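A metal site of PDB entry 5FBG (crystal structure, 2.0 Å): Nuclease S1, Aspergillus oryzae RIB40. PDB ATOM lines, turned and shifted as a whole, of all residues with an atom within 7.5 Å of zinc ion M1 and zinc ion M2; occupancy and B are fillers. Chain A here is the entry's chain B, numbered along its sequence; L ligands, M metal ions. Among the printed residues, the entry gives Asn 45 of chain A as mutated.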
ATOM      1  N   TRP A   1       4.495 -17.770   0.672  1.00  0.00           N
ATOM      2  CA  TRP A   1       3.825 -18.949   1.192  1.00  0.00           C
ATOM      3  C   TRP A   1       3.599 -19.936   0.064  1.00  0.00           C
ATOM      4  O   TRP A   1       3.530 -19.577  -1.104  1.00  0.00           O
ATOM      5  CB  TRP A   1       2.439 -18.639   1.837  1.00  0.00           C
ATOM      6  CG  TRP A   1       2.409 -17.535   2.854  1.00  0.00           C
ATOM      7  CD1 TRP A   1       2.027 -16.247   2.644  1.00  0.00           C
ATOM      8  CD2 TRP A   1       2.914 -17.590   4.199  1.00  0.00           C
ATOM      9  NE1 TRP A   1       2.190 -15.496   3.825  1.00  0.00           N
ATOM     10  CE2 TRP A   1       2.773 -16.304   4.756  1.00  0.00           C
ATOM     11  CE3 TRP A   1       3.512 -18.601   4.973  1.00  0.00           C
ATOM     12  CZ2 TRP A   1       3.102 -16.012   6.097  1.00  0.00           C
ATOM     13  CZ3 TRP A   1       3.872 -18.326   6.269  1.00  0.00           C
ATOM     14  CH2 TRP A   1       3.684 -17.007   6.819  1.00  0.00           C
ATOM     15  N   GLY A   2       3.404 -21.178   0.471  1.00  0.00           N
ATOM     16  CA  GLY A   2       2.886 -22.240  -0.409  1.00  0.00           C
ATOM     17  C   GLY A   2       1.387 -22.056  -0.591  1.00  0.00           C
ATOM     18  O   GLY A   2       0.795 -21.061  -0.127  1.00  0.00           O
ATOM     19  N   ASN A   3       0.772 -23.037  -1.221  1.00  0.00           N
ATOM     20  CA  ASN A   3      -0.655 -22.936  -1.556  1.00  0.00           C
ATOM     21  C   ASN A   3      -1.578 -22.740  -0.346  1.00  0.00           C
ATOM     22  O   ASN A   3      -2.465 -21.905  -0.358  1.00  0.00           O
ATOM     23  CB  ASN A   3      -1.116 -24.200  -2.328  1.00  0.00           C
ATOM     24  CG  ASN A   3      -0.413 -24.330  -3.673  1.00  0.00           C
ATOM     25  OD1 ASN A   3      -0.046 -23.345  -4.240  1.00  0.00           O
ATOM     26  ND2 ASN A   3      -0.215 -25.558  -4.149  1.00  0.00           N
ATOM     27  N   GLY A   5      -0.964 -21.486   2.639  1.00  0.00           N
ATOM     28  CA  GLY A   5      -0.855 -20.119   3.207  1.00  0.00           C
ATOM     29  C   GLY A   5      -1.600 -19.081   2.410  1.00  0.00           C
ATOM     30  O   GLY A   5      -2.382 -18.325   2.958  1.00  0.00           O
ATOM     31  N   HIS A   6      -1.422 -19.094   1.092  1.00  0.00           N
ATOM     32  CA  HIS A   6      -2.119 -18.156   0.252  1.00  0.00           C
ATOM     33  C   HIS A   6      -3.636 -18.294   0.288  1.00  0.00           C
ATOM     34  O   HIS A   6      -4.356 -17.280   0.289  1.00  0.00           O
ATOM     35  CB  HIS A   6      -1.641 -18.219  -1.198  1.00  0.00           C
ATOM     36  CG  HIS A   6      -0.298 -17.636  -1.381  1.00  0.00           C
ATOM     37  ND1 HIS A   6      -0.095 -16.284  -1.263  1.00  0.00           N
ATOM     38  CD2 HIS A   6       0.927 -18.203  -1.515  1.00  0.00           C
ATOM     39  CE1 HIS A   6       1.194 -16.036  -1.377  1.00  0.00           C
ATOM     40  NE2 HIS A   6       1.845 -17.176  -1.496  1.00  0.00           N
ATOM     41  N   ALA A  41      -5.588 -17.343  -5.499  1.00  0.00           N
ATOM     42  CA  ALA A  41      -4.546 -16.907  -4.555  1.00  0.00           C
ATOM     43  C   ALA A  41      -3.162 -17.447  -4.879  1.00  0.00           C
ATOM     44  O   ALA A  41      -2.177 -16.898  -4.380  1.00  0.00           O
ATOM     45  CB  ALA A  41      -4.912 -17.262  -3.125  1.00  0.00           C
ATOM     46  N   THR A  42      -3.097 -18.522  -5.633  1.00  0.00           N
ATOM     47  CA  THR A  42      -1.828 -19.132  -6.048  1.00  0.00           C
ATOM     48  C   THR A  42      -1.489 -18.877  -7.504  1.00  0.00           C
ATOM     49  O   THR A  42      -0.361 -19.204  -7.932  1.00  0.00           O
ATOM     50  CB  THR A  42      -1.788 -20.649  -5.849  1.00  0.00           C
ATOM     51  OG1 THR A  42      -2.771 -21.292  -6.635  1.00  0.00           O
ATOM     52  CG2 THR A  42      -2.157 -20.955  -4.470  1.00  0.00           C
ATOM     53  N   ALA A  44      -0.402 -16.394  -9.204  1.00  0.00           N
ATOM     54  CA  ALA A  44       0.824 -15.702  -9.511  1.00  0.00           C
ATOM     55  C   ALA A  44       2.022 -16.670  -9.588  1.00  0.00           C
ATOM     56  O   ALA A  44       2.957 -16.433 -10.336  1.00  0.00           O
ATOM     57  CB  ALA A  44       1.076 -14.505  -8.572  1.00  0.00           C
ATOM     58  N   ASN A  45       2.002 -17.685  -8.759  1.00  0.00           N
ATOM     59  CA  ASN A  45       3.016 -18.682  -8.743  1.00  0.00           C
ATOM     60  C   ASN A  45       3.006 -19.549 -10.030  1.00  0.00           C
ATOM     61  O   ASN A  45       4.050 -19.740 -10.627  1.00  0.00           O
ATOM     62  CB  ASN A  45       2.973 -19.560  -7.488  1.00  0.00           C
ATOM     63  CG  ASN A  45       3.604 -18.898  -6.263  1.00  0.00           C
ATOM     64  OD1 ASN A  45       4.255 -17.856  -6.342  1.00  0.00           O
ATOM     65  ND2 ASN A  45       3.299 -19.436  -5.111  1.00  0.00           N
ATOM     66  N   LYS A  48       4.352 -17.182 -12.900  1.00  0.00           N
ATOM     67  CA  LYS A  48       5.786 -16.851 -12.926  1.00  0.00           C
ATOM     68  C   LYS A  48       6.691 -17.911 -13.650  1.00  0.00           C
ATOM     69  O   LYS A  48       7.847 -17.609 -13.984  1.00  0.00           O
ATOM     70  CB  LYS A  48       6.316 -16.523 -11.533  1.00  0.00           C
ATOM     71  CG  LYS A  48       6.543 -17.724 -10.645  1.00  0.00           C
ATOM     72  CD  LYS A  48       6.821 -17.239  -9.240  1.00  0.00           C
ATOM     73  CE  LYS A  48       7.183 -18.292  -8.216  1.00  0.00           C
ATOM     74  NZ  LYS A  48       7.290 -17.706  -6.844  1.00  0.00           N
ATOM     75  N   LYS A  57       8.566 -12.909 -11.480  1.00  0.00           N
ATOM     76  CA  LYS A  57       9.191 -13.624 -10.349  1.00  0.00           C
ATOM     77  C   LYS A  57       9.670 -12.728  -9.197  1.00  0.00           C
ATOM     78  O   LYS A  57       9.476 -13.085  -8.070  1.00  0.00           O
ATOM     79  CB  LYS A  57      10.379 -14.495 -10.763  1.00  0.00           C
ATOM     80  CG  LYS A  57      10.008 -15.842 -11.271  1.00  0.00           C
ATOM     81  CD  LYS A  57      11.269 -16.630 -11.595  1.00  0.00           C
ATOM     82  CE  LYS A  57      10.852 -18.001 -12.110  1.00  0.00           C
ATOM     83  NZ  LYS A  57      12.027 -18.878 -12.362  1.00  0.00           N
ATOM     84  N   TYR A  59       8.476  -9.980  -8.230  1.00  0.00           N
ATOM     85  CA  TYR A  59       7.338  -9.310  -7.609  1.00  0.00           C
ATOM     86  C   TYR A  59       6.834 -10.015  -6.346  1.00  0.00           C
ATOM     87  O   TYR A  59       5.986  -9.479  -5.673  1.00  0.00           O
ATOM     88  CB  TYR A  59       6.182  -9.148  -8.567  1.00  0.00           C
ATOM     89  CG  TYR A  59       6.433  -8.351  -9.855  1.00  0.00           C
ATOM     90  CD1 TYR A  59       7.635  -7.640 -10.102  1.00  0.00           C
ATOM     91  CD2 TYR A  59       5.445  -8.285 -10.831  1.00  0.00           C
ATOM     92  CE1 TYR A  59       7.831  -6.909 -11.284  1.00  0.00           C
ATOM     93  CE2 TYR A  59       5.629  -7.563 -11.994  1.00  0.00           C
ATOM     94  CZ  TYR A  59       6.803  -6.879 -12.223  1.00  0.00           C
ATOM     95  OH  TYR A  59       6.945  -6.158 -13.371  1.00  0.00           O
ATOM     96  N   HIS A  60       7.424 -11.156  -6.002  1.00  0.00           N
ATOM     97  CA  HIS A  60       6.983 -11.938  -4.844  1.00  0.00           C
ATOM     98  C   HIS A  60       7.669 -11.566  -3.512  1.00  0.00           C
ATOM     99  O   HIS A  60       7.242 -12.058  -2.436  1.00  0.00           O
ATOM    100  CB  HIS A  60       7.100 -13.432  -5.170  1.00  0.00           C
ATOM    101  CG  HIS A  60       6.162 -13.864  -6.255  1.00  0.00           C
ATOM    102  ND1 HIS A  60       5.215 -14.849  -6.078  1.00  0.00           N
ATOM    103  CD2 HIS A  60       6.041 -13.454  -7.553  1.00  0.00           C
ATOM    104  CE1 HIS A  60       4.519 -14.993  -7.188  1.00  0.00           C
ATOM    105  NE2 HIS A  60       5.019 -14.178  -8.108  1.00  0.00           N
ATOM    106  N   PHE A  61       8.724 -10.729  -3.587  1.00  0.00           N
ATOM    107  CA  PHE A  61       9.580 -10.486  -2.444  1.00  0.00           C
ATOM    108  C   PHE A  61      10.267  -9.111  -2.538  1.00  0.00           C
ATOM    109  O   PHE A  61      10.188  -8.419  -3.563  1.00  0.00           O
ATOM    110  CB  PHE A  61      10.574 -11.654  -2.203  1.00  0.00           C
ATOM    111  CG  PHE A  61      11.463 -11.943  -3.405  1.00  0.00           C
ATOM    112  CD1 PHE A  61      12.585 -11.163  -3.692  1.00  0.00           C
ATOM    113  CD2 PHE A  61      11.091 -12.947  -4.305  1.00  0.00           C
ATOM    114  CE1 PHE A  61      13.363 -11.423  -4.817  1.00  0.00           C
ATOM    115  CE2 PHE A  61      11.850 -13.197  -5.448  1.00  0.00           C
ATOM    116  CZ  PHE A  61      12.991 -12.434  -5.710  1.00  0.00           C
ATOM    117  N   HIS A 115      -2.309 -12.390  -4.113  1.00  0.00           N
ATOM    118  CA  HIS A 115      -1.133 -13.223  -3.834  1.00  0.00           C
ATOM    119  C   HIS A 115      -0.054 -12.482  -3.069  1.00  0.00           C
ATOM    120  O   HIS A 115       0.479 -12.959  -2.066  1.00  0.00           O
ATOM    121  CB  HIS A 115      -0.542 -13.823  -5.155  1.00  0.00           C
ATOM    122  CG  HIS A 115       0.618 -14.726  -4.944  1.00  0.00           C
ATOM    123  ND1 HIS A 115       0.465 -16.072  -4.667  1.00  0.00           N
ATOM    124  CD2 HIS A 115       1.954 -14.478  -4.893  1.00  0.00           C
ATOM    125  CE1 HIS A 115       1.652 -16.625  -4.507  1.00  0.00           C
ATOM    126  NE2 HIS A 115       2.582 -15.685  -4.645  1.00  0.00           N
ATOM    127  N   ILE A 116       0.250 -11.298  -3.567  1.00  0.00           N
ATOM    128  CA  ILE A 116       1.409 -10.577  -3.090  1.00  0.00           C
ATOM    129  C   ILE A 116       1.218  -9.986  -1.671  1.00  0.00           C
ATOM    130  O   ILE A 116       2.140 -10.042  -0.877  1.00  0.00           O
ATOM    131  CB  ILE A 116       1.861  -9.515  -4.102  1.00  0.00           C
ATOM    132  CG1 ILE A 116       2.356 -10.204  -5.353  1.00  0.00           C
ATOM    133  CG2 ILE A 116       3.012  -8.663  -3.554  1.00  0.00           C
ATOM    134  CD1 ILE A 116       2.539  -9.266  -6.529  1.00  0.00           C
ATOM    135  N   GLY A 118      -0.320 -11.544   0.544  1.00  0.00           N
ATOM    136  CA  GLY A 118       0.036 -12.721   1.308  1.00  0.00           C
ATOM    137  C   GLY A 118       1.555 -12.881   1.458  1.00  0.00           C
ATOM    138  O   GLY A 118       2.108 -12.997   2.573  1.00  0.00           O
ATOM    139  N   ASP A 119       2.247 -12.826   0.334  1.00  0.00           N
ATOM    140  CA  ASP A 119       3.715 -13.065   0.325  1.00  0.00           C
ATOM    141  C   ASP A 119       4.498 -12.058   1.167  1.00  0.00           C
ATOM    142  O   ASP A 119       5.461 -12.433   1.858  1.00  0.00           O
ATOM    143  CB  ASP A 119       4.238 -13.010  -1.111  1.00  0.00           C
ATOM    144  CG  ASP A 119       4.337 -14.358  -1.782  1.00  0.00           C
ATOM    145  OD1 ASP A 119       4.182 -15.421  -1.146  1.00  0.00           O
ATOM    146  OD2 ASP A 119       4.661 -14.289  -3.027  1.00  0.00           O
ATOM    147  N   ILE A 120       4.088 -10.808   1.117  1.00  0.00           N
ATOM    148  CA  ILE A 120       4.738  -9.748   1.946  1.00  0.00           C
ATOM    149  C   ILE A 120       4.804 -10.135   3.436  1.00  0.00           C
ATOM    150  O   ILE A 120       5.747  -9.755   4.164  1.00  0.00           O
ATOM    151  CB  ILE A 120       4.071  -8.375   1.721  1.00  0.00           C
ATOM    152  CG1 ILE A 120       4.406  -7.866   0.344  1.00  0.00           C
ATOM    153  CG2 ILE A 120       4.469  -7.340   2.804  1.00  0.00           C
ATOM    154  CD1 ILE A 120       3.501  -6.701  -0.126  1.00  0.00           C
ATOM    155  N   GLN A 122       5.096 -13.089   4.682  1.00  0.00           N
ATOM    156  CA  GLN A 122       5.977 -14.193   4.964  1.00  0.00           C
ATOM    157  C   GLN A 122       7.356 -13.505   5.203  1.00  0.00           C
ATOM    158  O   GLN A 122       7.919 -12.967   4.248  1.00  0.00           O
ATOM    159  CB  GLN A 122       6.014 -15.221   3.798  1.00  0.00           C
ATOM    160  CG  GLN A 122       6.403 -16.641   4.144  1.00  0.00           C
ATOM    161  CD  GLN A 122       7.912 -16.856   4.434  1.00  0.00           C
ATOM    162  OE1 GLN A 122       8.482 -16.273   5.363  1.00  0.00           O
ATOM    163  NE2 GLN A 122       8.556 -17.698   3.628  1.00  0.00           N
ATOM    164  N   HIS A 125      10.224 -13.434   2.764  1.00  0.00           N
ATOM    165  CA  HIS A 125       9.953 -12.670   1.552  1.00  0.00           C
ATOM    166  C   HIS A 125      10.328 -11.187   1.718  1.00  0.00           C
ATOM    167  O   HIS A 125      10.124 -10.403   0.775  1.00  0.00           O
ATOM    168  CB  HIS A 125       8.506 -12.763   1.141  1.00  0.00           C
ATOM    169  CG  HIS A 125       8.170 -14.022   0.424  1.00  0.00           C
ATOM    170  ND1 HIS A 125       7.799 -14.039  -0.885  1.00  0.00           N
ATOM    171  CD2 HIS A 125       8.205 -15.325   0.831  1.00  0.00           C
ATOM    172  CE1 HIS A 125       7.607 -15.295  -1.272  1.00  0.00           C
ATOM    173  NE2 HIS A 125       7.883 -16.085  -0.253  1.00  0.00           N
ATOM    174  N   HIS A 148      13.580 -21.278   3.889  1.00  0.00           N
ATOM    175  CA  HIS A 148      12.486 -20.581   3.264  1.00  0.00           C
ATOM    176  C   HIS A 148      11.279 -21.535   3.079  1.00  0.00           C
ATOM    177  O   HIS A 148      10.136 -21.201   3.333  1.00  0.00           O
ATOM    178  CB  HIS A 148      12.891 -20.021   1.906  1.00  0.00           C
ATOM    179  CG  HIS A 148      11.825 -19.196   1.266  1.00  0.00           C
ATOM    180  ND1 HIS A 148      11.927 -17.828   1.152  1.00  0.00           N
ATOM    181  CD2 HIS A 148      10.643 -19.535   0.687  1.00  0.00           C
ATOM    182  CE1 HIS A 148      10.848 -17.359   0.544  1.00  0.00           C
ATOM    183  NE2 HIS A 148      10.052 -18.376   0.265  1.00  0.00           N
ATOM    184  N   ASP A 152       7.337 -21.337   4.157  1.00  0.00           N
ATOM    185  CA  ASP A 152       6.284 -21.228   3.143  1.00  0.00           C
ATOM    186  C   ASP A 152       5.256 -22.360   3.307  1.00  0.00           C
ATOM    187  O   ASP A 152       4.072 -22.138   3.174  1.00  0.00           O
ATOM    188  CB  ASP A 152       6.875 -21.347   1.703  1.00  0.00           C
ATOM    189  CG  ASP A 152       7.141 -20.046   1.028  1.00  0.00           C
ATOM    190  OD1 ASP A 152       6.974 -18.918   1.573  1.00  0.00           O
ATOM    191  OD2 ASP A 152       7.604 -20.105  -0.138  1.00  0.00           O
HETATM  192  P1  LIG L   1       6.011 -17.961  -3.280  1.00  0.00           P
HETATM  193  O1  LIG L   1       6.602 -16.828  -4.091  1.00  0.00           O
HETATM  194  O2  LIG L   1       6.528 -18.163  -1.884  1.00  0.00           O
HETATM  195  O3  LIG L   1       4.582 -17.588  -3.170  1.00  0.00           O
HETATM  196  O4  LIG L   1       6.264 -19.308  -4.013  1.00  0.00           O
HETATM  197  O1  LG2 L   2      12.619 -21.087  -5.304  1.00  0.00           O
HETATM  198  C1  LG2 L   2      13.780 -21.288  -6.113  1.00  0.00           C
HETATM  199  C2  LG2 L   2      14.650 -20.058  -6.258  1.00  0.00           C
HETATM  200  O2  LG2 L   2      13.803 -18.910  -6.483  1.00  0.00           O
HETATM  201  C3  LG2 L   2      14.301 -17.777  -5.771  1.00  0.00           C
HETATM  202  N1  LG2 L   2      13.252 -17.358  -4.715  1.00  0.00           N
HETATM  203  C4  LG2 L   2      12.022 -17.906  -4.379  1.00  0.00           C
HETATM  204  N2  LG2 L   2      11.396 -17.229  -3.399  1.00  0.00           N
HETATM  205  C5  LG2 L   2      12.265 -16.182  -3.094  1.00  0.00           C
HETATM  206  C6  LG2 L   2      13.408 -16.250  -3.898  1.00  0.00           C
HETATM  207  N3  LG2 L   2      14.450 -15.368  -3.817  1.00  0.00           N
HETATM  208  C7  LG2 L   2      14.385 -14.402  -2.849  1.00  0.00           C
HETATM  209  N4  LG2 L   2      13.358 -14.267  -2.013  1.00  0.00           N
HETATM  210  C8  LG2 L   2      12.244 -15.105  -2.090  1.00  0.00           C
HETATM  211  O3  LG2 L   2      11.253 -14.908  -1.377  1.00  0.00           O
HETATM  212  N5  LG2 L   2      15.412 -13.617  -2.736  1.00  0.00           N
HETATM  213  C9  LG2 L   2      15.668 -18.189  -5.232  1.00  0.00           C
HETATM  214  C10 LG2 L   2      15.508 -19.690  -5.035  1.00  0.00           C
HETATM  215  O4  LG2 L   2      16.776 -20.349  -4.913  1.00  0.00           O
HETATM  216 ZN    ZN M   1       4.605 -15.882  -4.360  1.00  0.00          ZN
HETATM  217 ZN    ZN M   2       3.837 -17.432  -1.325  1.00  0.00          ZN
HETATM  218 ZN    ZN M   3       8.177 -18.196  -0.684  1.00  0.00          ZN
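Zinc ion M1 is bound by NE2 of His 115 (2.1 Å), OD2 of Asp 119 (2.1 Å), O3 of LIG L1 (2.1 Å), ND1 of His 60 (2.1 Å) and O1 of LIG L1 (2.2 Å). Slightly farther from zinc ion M1 lies the side-chain amide oxygen (OD1) of Asn 45 (2.8 Å).
Zinc ion M2 is bound by an oxygen (O3) of LIG L1 (2.0 Å), a ring nitrogen (NE2) of His 6 (2.0 Å), the side-chain carboxylate (OD1) of Asp 119 (2.0 Å), the backbone nitrogen (N) of Trp 1 (2.1 Å) and the backbone carbonyl oxygen (O) of Trp 1 (2.2 Å). Zinc ion M2 has five donor atoms within binding distance. Slightly farther from zinc ion M2 lies O2 of LIG L1 (2.8 Å).
Within 4 Å of zinc ion M2: Trp 1, His 6, His 115 and Asp 119.
Within 4 Å of zinc ion M1: Asn 45, His 60, His 115 and Asp 119.
OD1 of Asp 152 sits close to N of Trp 1. NE2 of His 115 lies close to OD1 of Asn 45, 3.2 Å away. O of His 60 lies within hydrogen-bond range of ND1 of His 125 (2.6 Å). NE1 of Trp 1 is in hydrogen-bond range of O of Gly 118 (2.8 Å). ND1 of His 60 lies close to OD1 of Asn 45 (3.2 Å). A ring nitrogen (ND1) of His 6 sits close to a ring nitrogen (ND1) of His 115 (3.5 Å). The side-chain amide oxygen of Asn 45 is in hydrogen-bond range of the side-chain amino group of Lys 48 (3.1 Å). ND1 of His 115 is in hydrogen-bond range of O of Ala 41 (2.8 Å).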
